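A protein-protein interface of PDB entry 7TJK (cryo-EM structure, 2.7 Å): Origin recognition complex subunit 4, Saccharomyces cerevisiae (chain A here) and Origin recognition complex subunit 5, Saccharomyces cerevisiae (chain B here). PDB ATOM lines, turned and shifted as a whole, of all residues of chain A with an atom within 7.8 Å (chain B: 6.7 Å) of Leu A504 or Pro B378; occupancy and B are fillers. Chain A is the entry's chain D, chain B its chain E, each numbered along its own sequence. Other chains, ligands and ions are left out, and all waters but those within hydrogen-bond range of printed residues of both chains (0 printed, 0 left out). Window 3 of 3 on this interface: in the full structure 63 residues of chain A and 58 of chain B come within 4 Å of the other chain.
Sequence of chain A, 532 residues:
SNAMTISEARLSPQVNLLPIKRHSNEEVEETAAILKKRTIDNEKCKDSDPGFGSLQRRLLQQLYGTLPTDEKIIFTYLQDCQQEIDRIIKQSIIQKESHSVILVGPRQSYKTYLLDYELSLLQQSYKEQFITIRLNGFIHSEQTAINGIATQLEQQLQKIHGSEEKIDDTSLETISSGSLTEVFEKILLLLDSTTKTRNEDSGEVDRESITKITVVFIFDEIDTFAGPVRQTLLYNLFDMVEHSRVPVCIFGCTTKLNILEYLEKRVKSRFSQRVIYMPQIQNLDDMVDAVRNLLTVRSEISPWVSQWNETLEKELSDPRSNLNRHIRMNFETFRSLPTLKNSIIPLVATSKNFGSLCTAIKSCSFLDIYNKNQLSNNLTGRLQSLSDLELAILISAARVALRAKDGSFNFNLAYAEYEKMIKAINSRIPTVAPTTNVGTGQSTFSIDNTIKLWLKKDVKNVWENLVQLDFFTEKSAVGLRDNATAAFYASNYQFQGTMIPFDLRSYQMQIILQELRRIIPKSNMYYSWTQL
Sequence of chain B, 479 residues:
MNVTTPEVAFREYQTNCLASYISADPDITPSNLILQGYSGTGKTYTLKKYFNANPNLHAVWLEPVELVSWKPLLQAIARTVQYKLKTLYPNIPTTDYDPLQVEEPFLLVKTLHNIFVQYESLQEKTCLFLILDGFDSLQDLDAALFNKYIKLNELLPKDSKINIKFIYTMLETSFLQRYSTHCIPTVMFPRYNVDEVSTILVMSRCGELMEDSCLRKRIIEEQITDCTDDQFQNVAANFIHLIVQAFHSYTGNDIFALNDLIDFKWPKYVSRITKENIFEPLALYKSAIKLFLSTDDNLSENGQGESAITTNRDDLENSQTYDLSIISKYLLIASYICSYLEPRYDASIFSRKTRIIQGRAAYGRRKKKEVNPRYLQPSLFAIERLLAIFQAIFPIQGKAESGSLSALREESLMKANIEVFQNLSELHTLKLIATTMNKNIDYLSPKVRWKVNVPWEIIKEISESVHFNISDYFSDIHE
The side-chain amide nitrogen (ND2) of Asn A410 sits at hydrogen-bond distance from the backbone carbonyl oxygen (O) of Tyr B375 (2.7 Å).
The side-chain amide nitrogen of Gln B377 sits at hydrogen-bond distance from the backbone carbonyl oxygen of Leu A504 (3.2 Å).
Among the printed residues, pairs that only touch across the chains: Leu A504 with Tyr B375 (3.3 Å), Leu A504 with Leu B376 (3.4 Å), Ile A500 with Gln B377 (3.4 Å), Asn A412 with Tyr B375 (3.6 Å), Pro A501 with Asn B453 (3.7 Å), Asp A503 with Pro B455 (3.8 Å), Leu A504 with Pro B378 (3.8 Å), Pro A501 with Pro B455 (3.9 Å) and Ser A506 with Gln B377 (3.997 Å).
Of the printed residues of chain B, Asn A412 touches Tyr B375.
Printed residues of chain B within 4 Å of Asp A503: Pro B455 (3.8 Å).
Of the printed residues of chain B, Leu A504 touches Tyr B375, Leu B376, Gln B377 and Pro B378.
Of the printed residues of chain A, Tyr B375 touches Asn A410 (2.7 Å), Asn A412 (3.6 Å) and Leu A504 (3.3 Å).
Printed residues of chain A within 4 Å of Gln B377: Ile A500 (3.4 Å), Leu A504 (3.2 Å) and Ser A506 (3.997 Å).
Of chain A, only Leu A504 (3.8 Å) comes within 4 Å of Pro B378.
Ser B379 touches none of the printed residues of chain A.
Of the printed residues of chain A, Asn B453 touches Pro A501.
The nearest printed residue of chain B that does not touch Leu A504 is Tyr B340 (4.001 Å).
The nearest residue of chain A that does not touch Pro B378 is Ile A500 (6.5 Å).
The nearest printed residue of chain A that does not touch Tyr B375 is Asp A503 (4.7 Å).
OD1 of Asn A410 sits close to N of Asn A412 (3.4 Å).
The side-chain amide nitrogen (ND2) of Asn A412 is in hydrogen-bond range of the backbone carbonyl oxygen (O) of Asp A503 (3.4 Å).
O of Leu B376 lies within hydrogen-bond range of OH of Tyr B340.
Of the 14 printed residues of chain A, 7 touch a printed residue of chain B.
Of the 16 printed residues of chain B, 6 touch a printed residue of chain A.
Hydrophobic or aromatic side chains of chain B that line the printed part of chain A: Tyr B375, Pro B378 and Pro B455.
Among the printed residues, 11 pairs touch across the chains.
Among the printed residues, no Asp or Glu carboxylate lies within 4 Å of a Lys or Arg side-chain nitrogen of the other chain.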
ATOM      1  N   PHE A 409     -26.599  14.397 -17.975  1.00  0.00           N
ATOM      2  CA  PHE A 409     -25.202  14.003 -17.863  1.00  0.00           C
ATOM      3  C   PHE A 409     -25.114  12.883 -16.838  1.00  0.00           C
ATOM      4  O   PHE A 409     -26.070  12.606 -16.112  1.00  0.00           O
ATOM      5  CB  PHE A 409     -24.303  15.188 -17.469  1.00  0.00           C
ATOM      6  CG  PHE A 409     -24.695  15.858 -16.178  1.00  0.00           C
ATOM      7  CD1 PHE A 409     -25.647  16.868 -16.162  1.00  0.00           C
ATOM      8  CD2 PHE A 409     -24.096  15.494 -14.980  1.00  0.00           C
ATOM      9  CE1 PHE A 409     -26.008  17.477 -14.982  1.00  0.00           C
ATOM     10  CE2 PHE A 409     -24.457  16.104 -13.797  1.00  0.00           C
ATOM     11  CZ  PHE A 409     -25.410  17.089 -13.798  1.00  0.00           C
ATOM     12  N   ASN A 410     -23.950  12.243 -16.783  1.00  0.00           N
ATOM     13  CA  ASN A 410     -23.666  11.269 -15.740  1.00  0.00           C
ATOM     14  C   ASN A 410     -22.263  11.512 -15.198  1.00  0.00           C
ATOM     15  O   ASN A 410     -21.608  12.503 -15.531  1.00  0.00           O
ATOM     16  CB  ASN A 410     -23.867   9.826 -16.239  1.00  0.00           C
ATOM     17  CG  ASN A 410     -23.157   9.532 -17.558  1.00  0.00           C
ATOM     18  OD1 ASN A 410     -22.146  10.138 -17.900  1.00  0.00           O
ATOM     19  ND2 ASN A 410     -23.699   8.578 -18.304  1.00  0.00           N
ATOM     20  N   PHE A 411     -21.814  10.590 -14.344  1.00  0.00           N
ATOM     21  CA  PHE A 411     -20.503  10.702 -13.713  1.00  0.00           C
ATOM     22  C   PHE A 411     -19.369  10.542 -14.720  1.00  0.00           C
ATOM     23  O   PHE A 411     -18.331  11.202 -14.591  1.00  0.00           O
ATOM     24  CB  PHE A 411     -20.390   9.656 -12.602  1.00  0.00           C
ATOM     25  CG  PHE A 411     -19.097   9.698 -11.845  1.00  0.00           C
ATOM     26  CD1 PHE A 411     -18.907  10.625 -10.836  1.00  0.00           C
ATOM     27  CD2 PHE A 411     -18.080   8.795 -12.126  1.00  0.00           C
ATOM     28  CE1 PHE A 411     -17.725  10.661 -10.131  1.00  0.00           C
ATOM     29  CE2 PHE A 411     -16.890   8.831 -11.428  1.00  0.00           C
ATOM     30  CZ  PHE A 411     -16.712   9.764 -10.428  1.00  0.00           C
ATOM     31  N   ASN A 412     -19.554   9.679 -15.724  1.00  0.00           N
ATOM     32  CA  ASN A 412     -18.480   9.363 -16.662  1.00  0.00           C
ATOM     33  C   ASN A 412     -18.157  10.541 -17.574  1.00  0.00           C
ATOM     34  O   ASN A 412     -16.981  10.871 -17.777  1.00  0.00           O
ATOM     35  CB  ASN A 412     -18.860   8.135 -17.487  1.00  0.00           C
ATOM     36  CG  ASN A 412     -18.871   6.862 -16.665  1.00  0.00           C
ATOM     37  OD1 ASN A 412     -18.108   6.719 -15.711  1.00  0.00           O
ATOM     38  ND2 ASN A 412     -19.744   5.932 -17.029  1.00  0.00           N
ATOM     39  N   TRP A 463     -18.821  13.729  -5.938  1.00  0.00           N
ATOM     40  CA  TRP A 463     -20.083  13.626  -6.663  1.00  0.00           C
ATOM     41  C   TRP A 463     -21.257  13.410  -5.716  1.00  0.00           C
ATOM     42  O   TRP A 463     -22.323  14.020  -5.882  1.00  0.00           O
ATOM     43  CB  TRP A 463     -19.987  12.480  -7.666  1.00  0.00           C
ATOM     44  CG  TRP A 463     -21.114  12.395  -8.627  1.00  0.00           C
ATOM     45  CD1 TRP A 463     -22.234  11.628  -8.515  1.00  0.00           C
ATOM     46  CD2 TRP A 463     -21.226  13.092  -9.867  1.00  0.00           C
ATOM     47  NE1 TRP A 463     -23.042  11.810  -9.609  1.00  0.00           N
ATOM     48  CE2 TRP A 463     -22.442  12.703 -10.456  1.00  0.00           C
ATOM     49  CE3 TRP A 463     -20.414  14.008 -10.537  1.00  0.00           C
ATOM     50  CZ2 TRP A 463     -22.866  13.201 -11.681  1.00  0.00           C
ATOM     51  CZ3 TRP A 463     -20.834  14.498 -11.749  1.00  0.00           C
ATOM     52  CH2 TRP A 463     -22.049  14.095 -12.310  1.00  0.00           C
ATOM     53  N   GLY A 497     -33.653   4.391 -11.610  1.00  0.00           N
ATOM     54  CA  GLY A 497     -32.395   5.028 -11.274  1.00  0.00           C
ATOM     55  C   GLY A 497     -31.686   4.430 -10.076  1.00  0.00           C
ATOM     56  O   GLY A 497     -30.469   4.603  -9.952  1.00  0.00           O
ATOM     57  N   ILE A 500     -29.502   0.877 -11.380  1.00  0.00           N
ATOM     58  CA  ILE A 500     -28.361   0.941 -12.288  1.00  0.00           C
ATOM     59  C   ILE A 500     -27.174   1.474 -11.491  1.00  0.00           C
ATOM     60  O   ILE A 500     -27.382   2.068 -10.422  1.00  0.00           O
ATOM     61  CB  ILE A 500     -28.686   1.805 -13.520  1.00  0.00           C
ATOM     62  CG1 ILE A 500     -28.794   3.280 -13.141  1.00  0.00           C
ATOM     63  CG2 ILE A 500     -29.971   1.329 -14.182  1.00  0.00           C
ATOM     64  CD1 ILE A 500     -28.815   4.196 -14.327  1.00  0.00           C
ATOM     65  N   PRO A 501     -25.928   1.244 -11.922  1.00  0.00           N
ATOM     66  CA  PRO A 501     -24.782   1.826 -11.212  1.00  0.00           C
ATOM     67  C   PRO A 501     -24.770   3.346 -11.284  1.00  0.00           C
ATOM     68  O   PRO A 501     -25.311   3.958 -12.207  1.00  0.00           O
ATOM     69  CB  PRO A 501     -23.567   1.226 -11.934  1.00  0.00           C
ATOM     70  CG  PRO A 501     -24.102   0.638 -13.203  1.00  0.00           C
ATOM     71  CD  PRO A 501     -25.491   0.213 -12.879  1.00  0.00           C
ATOM     72  N   PHE A 502     -24.140   3.950 -10.267  1.00  0.00           N
ATOM     73  CA  PHE A 502     -24.185   5.394 -10.059  1.00  0.00           C
ATOM     74  C   PHE A 502     -23.503   6.178 -11.173  1.00  0.00           C
ATOM     75  O   PHE A 502     -23.830   7.351 -11.375  1.00  0.00           O
ATOM     76  CB  PHE A 502     -23.549   5.749  -8.709  1.00  0.00           C
ATOM     77  CG  PHE A 502     -22.053   5.925  -8.764  1.00  0.00           C
ATOM     78  CD1 PHE A 502     -21.221   4.823  -8.866  1.00  0.00           C
ATOM     79  CD2 PHE A 502     -21.481   7.190  -8.699  1.00  0.00           C
ATOM     80  CE1 PHE A 502     -19.846   4.977  -8.918  1.00  0.00           C
ATOM     81  CE2 PHE A 502     -20.110   7.349  -8.757  1.00  0.00           C
ATOM     82  CZ  PHE A 502     -19.293   6.241  -8.863  1.00  0.00           C
ATOM     83  N   ASP A 503     -22.561   5.566 -11.888  1.00  0.00           N
ATOM     84  CA  ASP A 503     -21.872   6.229 -12.984  1.00  0.00           C
ATOM     85  C   ASP A 503     -22.729   6.353 -14.239  1.00  0.00           C
ATOM     86  O   ASP A 503     -22.323   7.047 -15.176  1.00  0.00           O
ATOM     87  CB  ASP A 503     -20.559   5.493 -13.287  1.00  0.00           C
ATOM     88  CG  ASP A 503     -20.768   4.039 -13.693  1.00  0.00           C
ATOM     89  OD1 ASP A 503     -21.189   3.773 -14.837  1.00  0.00           O
ATOM     90  OD2 ASP A 503     -20.510   3.152 -12.852  1.00  0.00           O
ATOM     91  N   LEU A 504     -23.893   5.706 -14.278  1.00  0.00           N
ATOM     92  CA  LEU A 504     -24.794   5.780 -15.416  1.00  0.00           C
ATOM     93  C   LEU A 504     -26.103   6.495 -15.112  1.00  0.00           C
ATOM     94  O   LEU A 504     -26.940   6.619 -16.013  1.00  0.00           O
ATOM     95  CB  LEU A 504     -25.099   4.371 -15.945  1.00  0.00           C
ATOM     96  CG  LEU A 504     -23.977   3.646 -16.690  1.00  0.00           C
ATOM     97  CD1 LEU A 504     -24.500   2.388 -17.363  1.00  0.00           C
ATOM     98  CD2 LEU A 504     -23.329   4.561 -17.710  1.00  0.00           C
ATOM     99  N   ARG A 505     -26.313   6.956 -13.880  1.00  0.00           N
ATOM    100  CA  ARG A 505     -27.535   7.678 -13.545  1.00  0.00           C
ATOM    101  C   ARG A 505     -27.543   9.048 -14.209  1.00  0.00           C
ATOM    102  O   ARG A 505     -26.549   9.777 -14.170  1.00  0.00           O
ATOM    103  CB  ARG A 505     -27.672   7.832 -12.032  1.00  0.00           C
ATOM    104  CG  ARG A 505     -27.849   6.530 -11.280  1.00  0.00           C
ATOM    105  CD  ARG A 505     -27.867   6.762  -9.779  1.00  0.00           C
ATOM    106  NE  ARG A 505     -27.780   5.510  -9.039  1.00  0.00           N
ATOM    107  CZ  ARG A 505     -27.252   5.389  -7.829  1.00  0.00           C
ATOM    108  NH1 ARG A 505     -26.769   6.435  -7.178  1.00  0.00           N
ATOM    109  NH2 ARG A 505     -27.203   4.188  -7.259  1.00  0.00           N
ATOM    110  N   SER A 506     -28.671   9.397 -14.820  1.00  0.00           N
ATOM    111  CA  SER A 506     -28.811  10.690 -15.469  1.00  0.00           C
ATOM    112  C   SER A 506     -29.126  11.768 -14.440  1.00  0.00           C
ATOM    113  O   SER A 506     -29.961  11.576 -13.553  1.00  0.00           O
ATOM    114  CB  SER A 506     -29.908  10.636 -16.530  1.00  0.00           C
ATOM    115  OG  SER A 506     -29.601   9.685 -17.532  1.00  0.00           O
ATOM    116  N   TYR A 507     -28.446  12.902 -14.563  1.00  0.00           N
ATOM    117  CA  TYR A 507     -28.617  14.026 -13.656  1.00  0.00           C
ATOM    118  C   TYR A 507     -28.818  15.301 -14.459  1.00  0.00           C
ATOM    119  O   TYR A 507     -28.464  15.387 -15.636  1.00  0.00           O
ATOM    120  CB  TYR A 507     -27.418  14.183 -12.710  1.00  0.00           C
ATOM    121  CG  TYR A 507     -27.364  13.163 -11.598  1.00  0.00           C
ATOM    122  CD1 TYR A 507     -28.048  13.370 -10.407  1.00  0.00           C
ATOM    123  CD2 TYR A 507     -26.620  11.999 -11.735  1.00  0.00           C
ATOM    124  CE1 TYR A 507     -28.000  12.443  -9.386  1.00  0.00           C
ATOM    125  CE2 TYR A 507     -26.563  11.065 -10.718  1.00  0.00           C
ATOM    126  CZ  TYR A 507     -27.255  11.292  -9.547  1.00  0.00           C
ATOM    127  OH  TYR A 507     -27.202  10.367  -8.534  1.00  0.00           O
ATOM    128  N   SER B 335     -22.926 -10.509 -23.034  1.00  0.00           N
ATOM    129  CA  SER B 335     -23.979  -9.556 -22.697  1.00  0.00           C
ATOM    130  C   SER B 335     -23.508  -8.120 -22.869  1.00  0.00           C
ATOM    131  O   SER B 335     -24.254  -7.275 -23.377  1.00  0.00           O
ATOM    132  CB  SER B 335     -24.446  -9.793 -21.263  1.00  0.00           C
ATOM    133  OG  SER B 335     -24.758 -11.156 -21.038  1.00  0.00           O
ATOM    134  N   SER B 339     -24.924  -5.464 -25.528  1.00  0.00           N
ATOM    135  CA  SER B 339     -25.469  -4.200 -25.054  1.00  0.00           C
ATOM    136  C   SER B 339     -24.740  -2.995 -25.631  1.00  0.00           C
ATOM    137  O   SER B 339     -25.320  -1.906 -25.697  1.00  0.00           O
ATOM    138  CB  SER B 339     -25.419  -4.142 -23.529  1.00  0.00           C
ATOM    139  OG  SER B 339     -26.404  -4.975 -22.949  1.00  0.00           O
ATOM    140  N   TYR B 340     -23.483  -3.152 -26.047  1.00  0.00           N
ATOM    141  CA  TYR B 340     -22.705  -2.005 -26.505  1.00  0.00           C
ATOM    142  C   TYR B 340     -22.187  -2.143 -27.930  1.00  0.00           C
ATOM    143  O   TYR B 340     -21.279  -1.400 -28.320  1.00  0.00           O
ATOM    144  CB  TYR B 340     -21.557  -1.746 -25.531  1.00  0.00           C
ATOM    145  CG  TYR B 340     -22.042  -1.205 -24.210  1.00  0.00           C
ATOM    146  CD1 TYR B 340     -22.473   0.109 -24.096  1.00  0.00           C
ATOM    147  CD2 TYR B 340     -22.124  -2.020 -23.090  1.00  0.00           C
ATOM    148  CE1 TYR B 340     -22.930   0.606 -22.892  1.00  0.00           C
ATOM    149  CE2 TYR B 340     -22.578  -1.530 -21.881  1.00  0.00           C
ATOM    150  CZ  TYR B 340     -22.979  -0.216 -21.791  1.00  0.00           C
ATOM    151  OH  TYR B 340     -23.438   0.283 -20.595  1.00  0.00           O
ATOM    152  N   PRO B 373     -19.549   4.707 -26.497  1.00  0.00           N
ATOM    153  CA  PRO B 373     -20.829   4.170 -25.998  1.00  0.00           C
ATOM    154  C   PRO B 373     -20.789   3.585 -24.589  1.00  0.00           C
ATOM    155  O   PRO B 373     -21.860   3.391 -24.001  1.00  0.00           O
ATOM    156  CB  PRO B 373     -21.179   3.084 -27.026  1.00  0.00           C
ATOM    157  CG  PRO B 373     -20.328   3.387 -28.224  1.00  0.00           C
ATOM    158  CD  PRO B 373     -19.067   3.959 -27.667  1.00  0.00           C
ATOM    159  N   ARG B 374     -19.613   3.321 -24.020  1.00  0.00           N
ATOM    160  CA  ARG B 374     -19.520   2.820 -22.653  1.00  0.00           C
ATOM    161  C   ARG B 374     -19.874   3.868 -21.603  1.00  0.00           C
ATOM    162  O   ARG B 374     -20.028   3.513 -20.430  1.00  0.00           O
ATOM    163  CB  ARG B 374     -18.112   2.285 -22.352  1.00  0.00           C
ATOM    164  CG  ARG B 374     -17.772   0.908 -22.929  1.00  0.00           C
ATOM    165  CD  ARG B 374     -17.329   0.952 -24.385  1.00  0.00           C
ATOM    166  NE  ARG B 374     -16.164   1.813 -24.549  1.00  0.00           N
ATOM    167  CZ  ARG B 374     -14.911   1.422 -24.356  1.00  0.00           C
ATOM    168  NH1 ARG B 374     -14.622   0.184 -23.994  1.00  0.00           N
ATOM    169  NH2 ARG B 374     -13.926   2.299 -24.515  1.00  0.00           N
ATOM    170  N   TYR B 375     -19.990   5.143 -21.975  1.00  0.00           N
ATOM    171  CA  TYR B 375     -20.404   6.168 -21.028  1.00  0.00           C
ATOM    172  C   TYR B 375     -21.917   6.258 -20.875  1.00  0.00           C
ATOM    173  O   TYR B 375     -22.388   6.879 -19.918  1.00  0.00           O
ATOM    174  CB  TYR B 375     -19.855   7.536 -21.451  1.00  0.00           C
ATOM    175  CG  TYR B 375     -18.343   7.638 -21.458  1.00  0.00           C
ATOM    176  CD1 TYR B 375     -17.565   6.844 -20.621  1.00  0.00           C
ATOM    177  CD2 TYR B 375     -17.696   8.528 -22.305  1.00  0.00           C
ATOM    178  CE1 TYR B 375     -16.184   6.937 -20.627  1.00  0.00           C
ATOM    179  CE2 TYR B 375     -16.316   8.625 -22.318  1.00  0.00           C
ATOM    180  CZ  TYR B 375     -15.568   7.827 -21.478  1.00  0.00           C
ATOM    181  OH  TYR B 375     -14.197   7.922 -21.488  1.00  0.00           O
ATOM    182  N   LEU B 376     -22.683   5.663 -21.782  1.00  0.00           N
ATOM    183  CA  LEU B 376     -24.137   5.698 -21.747  1.00  0.00           C
ATOM    184  C   LEU B 376     -24.684   4.409 -21.140  1.00  0.00           C
ATOM    185  O   LEU B 376     -23.955   3.449 -20.885  1.00  0.00           O
ATOM    186  CB  LEU B 376     -24.726   5.940 -23.144  1.00  0.00           C
ATOM    187  CG  LEU B 376     -24.313   7.137 -24.018  1.00  0.00           C
ATOM    188  CD1 LEU B 376     -23.052   6.916 -24.846  1.00  0.00           C
ATOM    189  CD2 LEU B 376     -25.470   7.547 -24.925  1.00  0.00           C
ATOM    190  N   GLN B 377     -25.994   4.412 -20.895  1.00  0.00           N
ATOM    191  CA  GLN B 377     -26.709   3.250 -20.398  1.00  0.00           C
ATOM    192  C   GLN B 377     -26.763   2.165 -21.475  1.00  0.00           C
ATOM    193  O   GLN B 377     -26.809   2.472 -22.669  1.00  0.00           O
ATOM    194  CB  GLN B 377     -28.122   3.643 -19.973  1.00  0.00           C
ATOM    195  CG  GLN B 377     -28.170   4.566 -18.765  1.00  0.00           C
ATOM    196  CD  GLN B 377     -29.586   4.952 -18.380  1.00  0.00           C
ATOM    197  OE1 GLN B 377     -30.547   4.581 -19.057  1.00  0.00           O
ATOM    198  NE2 GLN B 377     -29.724   5.697 -17.290  1.00  0.00           N
ATOM    199  N   PRO B 378     -26.731   0.891 -21.079  1.00  0.00           N
ATOM    200  CA  PRO B 378     -26.701  -0.193 -22.068  1.00  0.00           C
ATOM    201  C   PRO B 378     -28.015  -0.339 -22.820  1.00  0.00           C
ATOM    202  O   PRO B 378     -29.094  -0.005 -22.326  1.00  0.00           O
ATOM    203  CB  PRO B 378     -26.417  -1.433 -21.216  1.00  0.00           C
ATOM    204  CG  PRO B 378     -26.961  -1.085 -19.884  1.00  0.00           C
ATOM    205  CD  PRO B 378     -26.624   0.361 -19.707  1.00  0.00           C
ATOM    206  N   SER B 379     -27.902  -0.849 -24.042  1.00  0.00           N
ATOM    207  CA  SER B 379     -29.055  -1.128 -24.881  1.00  0.00           C
ATOM    208  C   SER B 379     -29.593  -2.529 -24.596  1.00  0.00           C
ATOM    209  O   SER B 379     -28.978  -3.330 -23.889  1.00  0.00           O
ATOM    210  CB  SER B 379     -28.690  -0.981 -26.359  1.00  0.00           C
ATOM    211  OG  SER B 379     -29.717  -1.489 -27.193  1.00  0.00           O
ATOM    212  N   LEU B 380     -30.758  -2.821 -25.164  1.00  0.00           N
ATOM    213  CA  LEU B 380     -31.472  -4.060 -24.892  1.00  0.00           C
ATOM    214  C   LEU B 380     -31.293  -5.055 -26.033  1.00  0.00           C
ATOM    215  O   LEU B 380     -31.293  -4.674 -27.207  1.00  0.00           O
ATOM    216  CB  LEU B 380     -32.957  -3.784 -24.658  1.00  0.00           C
ATOM    217  CG  LEU B 380     -33.289  -2.935 -23.429  1.00  0.00           C
ATOM    218  CD1 LEU B 380     -34.690  -2.349 -23.539  1.00  0.00           C
ATOM    219  CD2 LEU B 380     -33.138  -3.751 -22.159  1.00  0.00           C
ATOM    220  N   LYS B 451     -30.388  -6.752 -20.644  1.00  0.00           N
ATOM    221  CA  LYS B 451     -29.285  -5.803 -20.663  1.00  0.00           C
ATOM    222  C   LYS B 451     -28.283  -6.164 -19.576  1.00  0.00           C
ATOM    223  O   LYS B 451     -28.612  -6.828 -18.592  1.00  0.00           O
ATOM    224  CB  LYS B 451     -29.768  -4.355 -20.490  1.00  0.00           C
ATOM    225  CG  LYS B 451     -30.314  -4.025 -19.117  1.00  0.00           C
ATOM    226  CD  LYS B 451     -31.066  -2.708 -19.135  1.00  0.00           C
ATOM    227  CE  LYS B 451     -31.812  -2.480 -17.831  1.00  0.00           C
ATOM    228  NZ  LYS B 451     -32.598  -1.218 -17.865  1.00  0.00           N
ATOM    229  N   VAL B 452     -27.045  -5.730 -19.781  1.00  0.00           N
ATOM    230  CA  VAL B 452     -25.991  -5.933 -18.801  1.00  0.00           C
ATOM    231  C   VAL B 452     -26.160  -4.891 -17.698  1.00  0.00           C
ATOM    232  O   VAL B 452     -26.641  -3.778 -17.923  1.00  0.00           O
ATOM    233  CB  VAL B 452     -24.589  -5.878 -19.468  1.00  0.00           C
ATOM    234  CG1 VAL B 452     -24.256  -4.484 -19.997  1.00  0.00           C
ATOM    235  CG2 VAL B 452     -23.495  -6.417 -18.554  1.00  0.00           C
ATOM    236  N   ASN B 453     -25.816  -5.273 -16.470  1.00  0.00           N
ATOM    237  CA  ASN B 453     -26.030  -4.421 -15.309  1.00  0.00           C
ATOM    238  C   ASN B 453     -24.706  -4.036 -14.666  1.00  0.00           C
ATOM    239  O   ASN B 453     -24.669  -3.305 -13.672  1.00  0.00           O
ATOM    240  CB  ASN B 453     -26.942  -5.107 -14.293  1.00  0.00           C
ATOM    241  CG  ASN B 453     -27.751  -4.118 -13.473  1.00  0.00           C
ATOM    242  OD1 ASN B 453     -27.732  -2.916 -13.733  1.00  0.00           O
ATOM    243  ND2 ASN B 453     -28.465  -4.623 -12.476  1.00  0.00           N
ATOM    244  N   VAL B 454     -23.594  -4.511 -15.221  1.00  0.00           N
ATOM    245  CA  VAL B 454     -22.288  -4.214 -14.637  1.00  0.00           C
ATOM    246  C   VAL B 454     -21.546  -3.190 -15.494  1.00  0.00           C
ATOM    247  O   VAL B 454     -21.762  -3.123 -16.714  1.00  0.00           O
ATOM    248  CB  VAL B 454     -21.465  -5.499 -14.431  1.00  0.00           C
ATOM    249  CG1 VAL B 454     -22.244  -6.480 -13.585  1.00  0.00           C
ATOM    250  CG2 VAL B 454     -21.082  -6.142 -15.750  1.00  0.00           C
ATOM    251  N   PRO B 455     -20.714  -2.344 -14.897  1.00  0.00           N
ATOM    252  CA  PRO B 455     -19.916  -1.386 -15.671  1.00  0.00           C
ATOM    253  C   PRO B 455     -18.674  -2.033 -16.281  1.00  0.00           C
ATOM    254  O   PRO B 455     -18.471  -3.245 -16.232  1.00  0.00           O
ATOM    255  CB  PRO B 455     -19.531  -0.321 -14.635  1.00  0.00           C
ATOM    256  CG  PRO B 455     -20.418  -0.551 -13.464  1.00  0.00           C
ATOM    257  CD  PRO B 455     -20.744  -2.001 -13.467  1.00  0.00           C
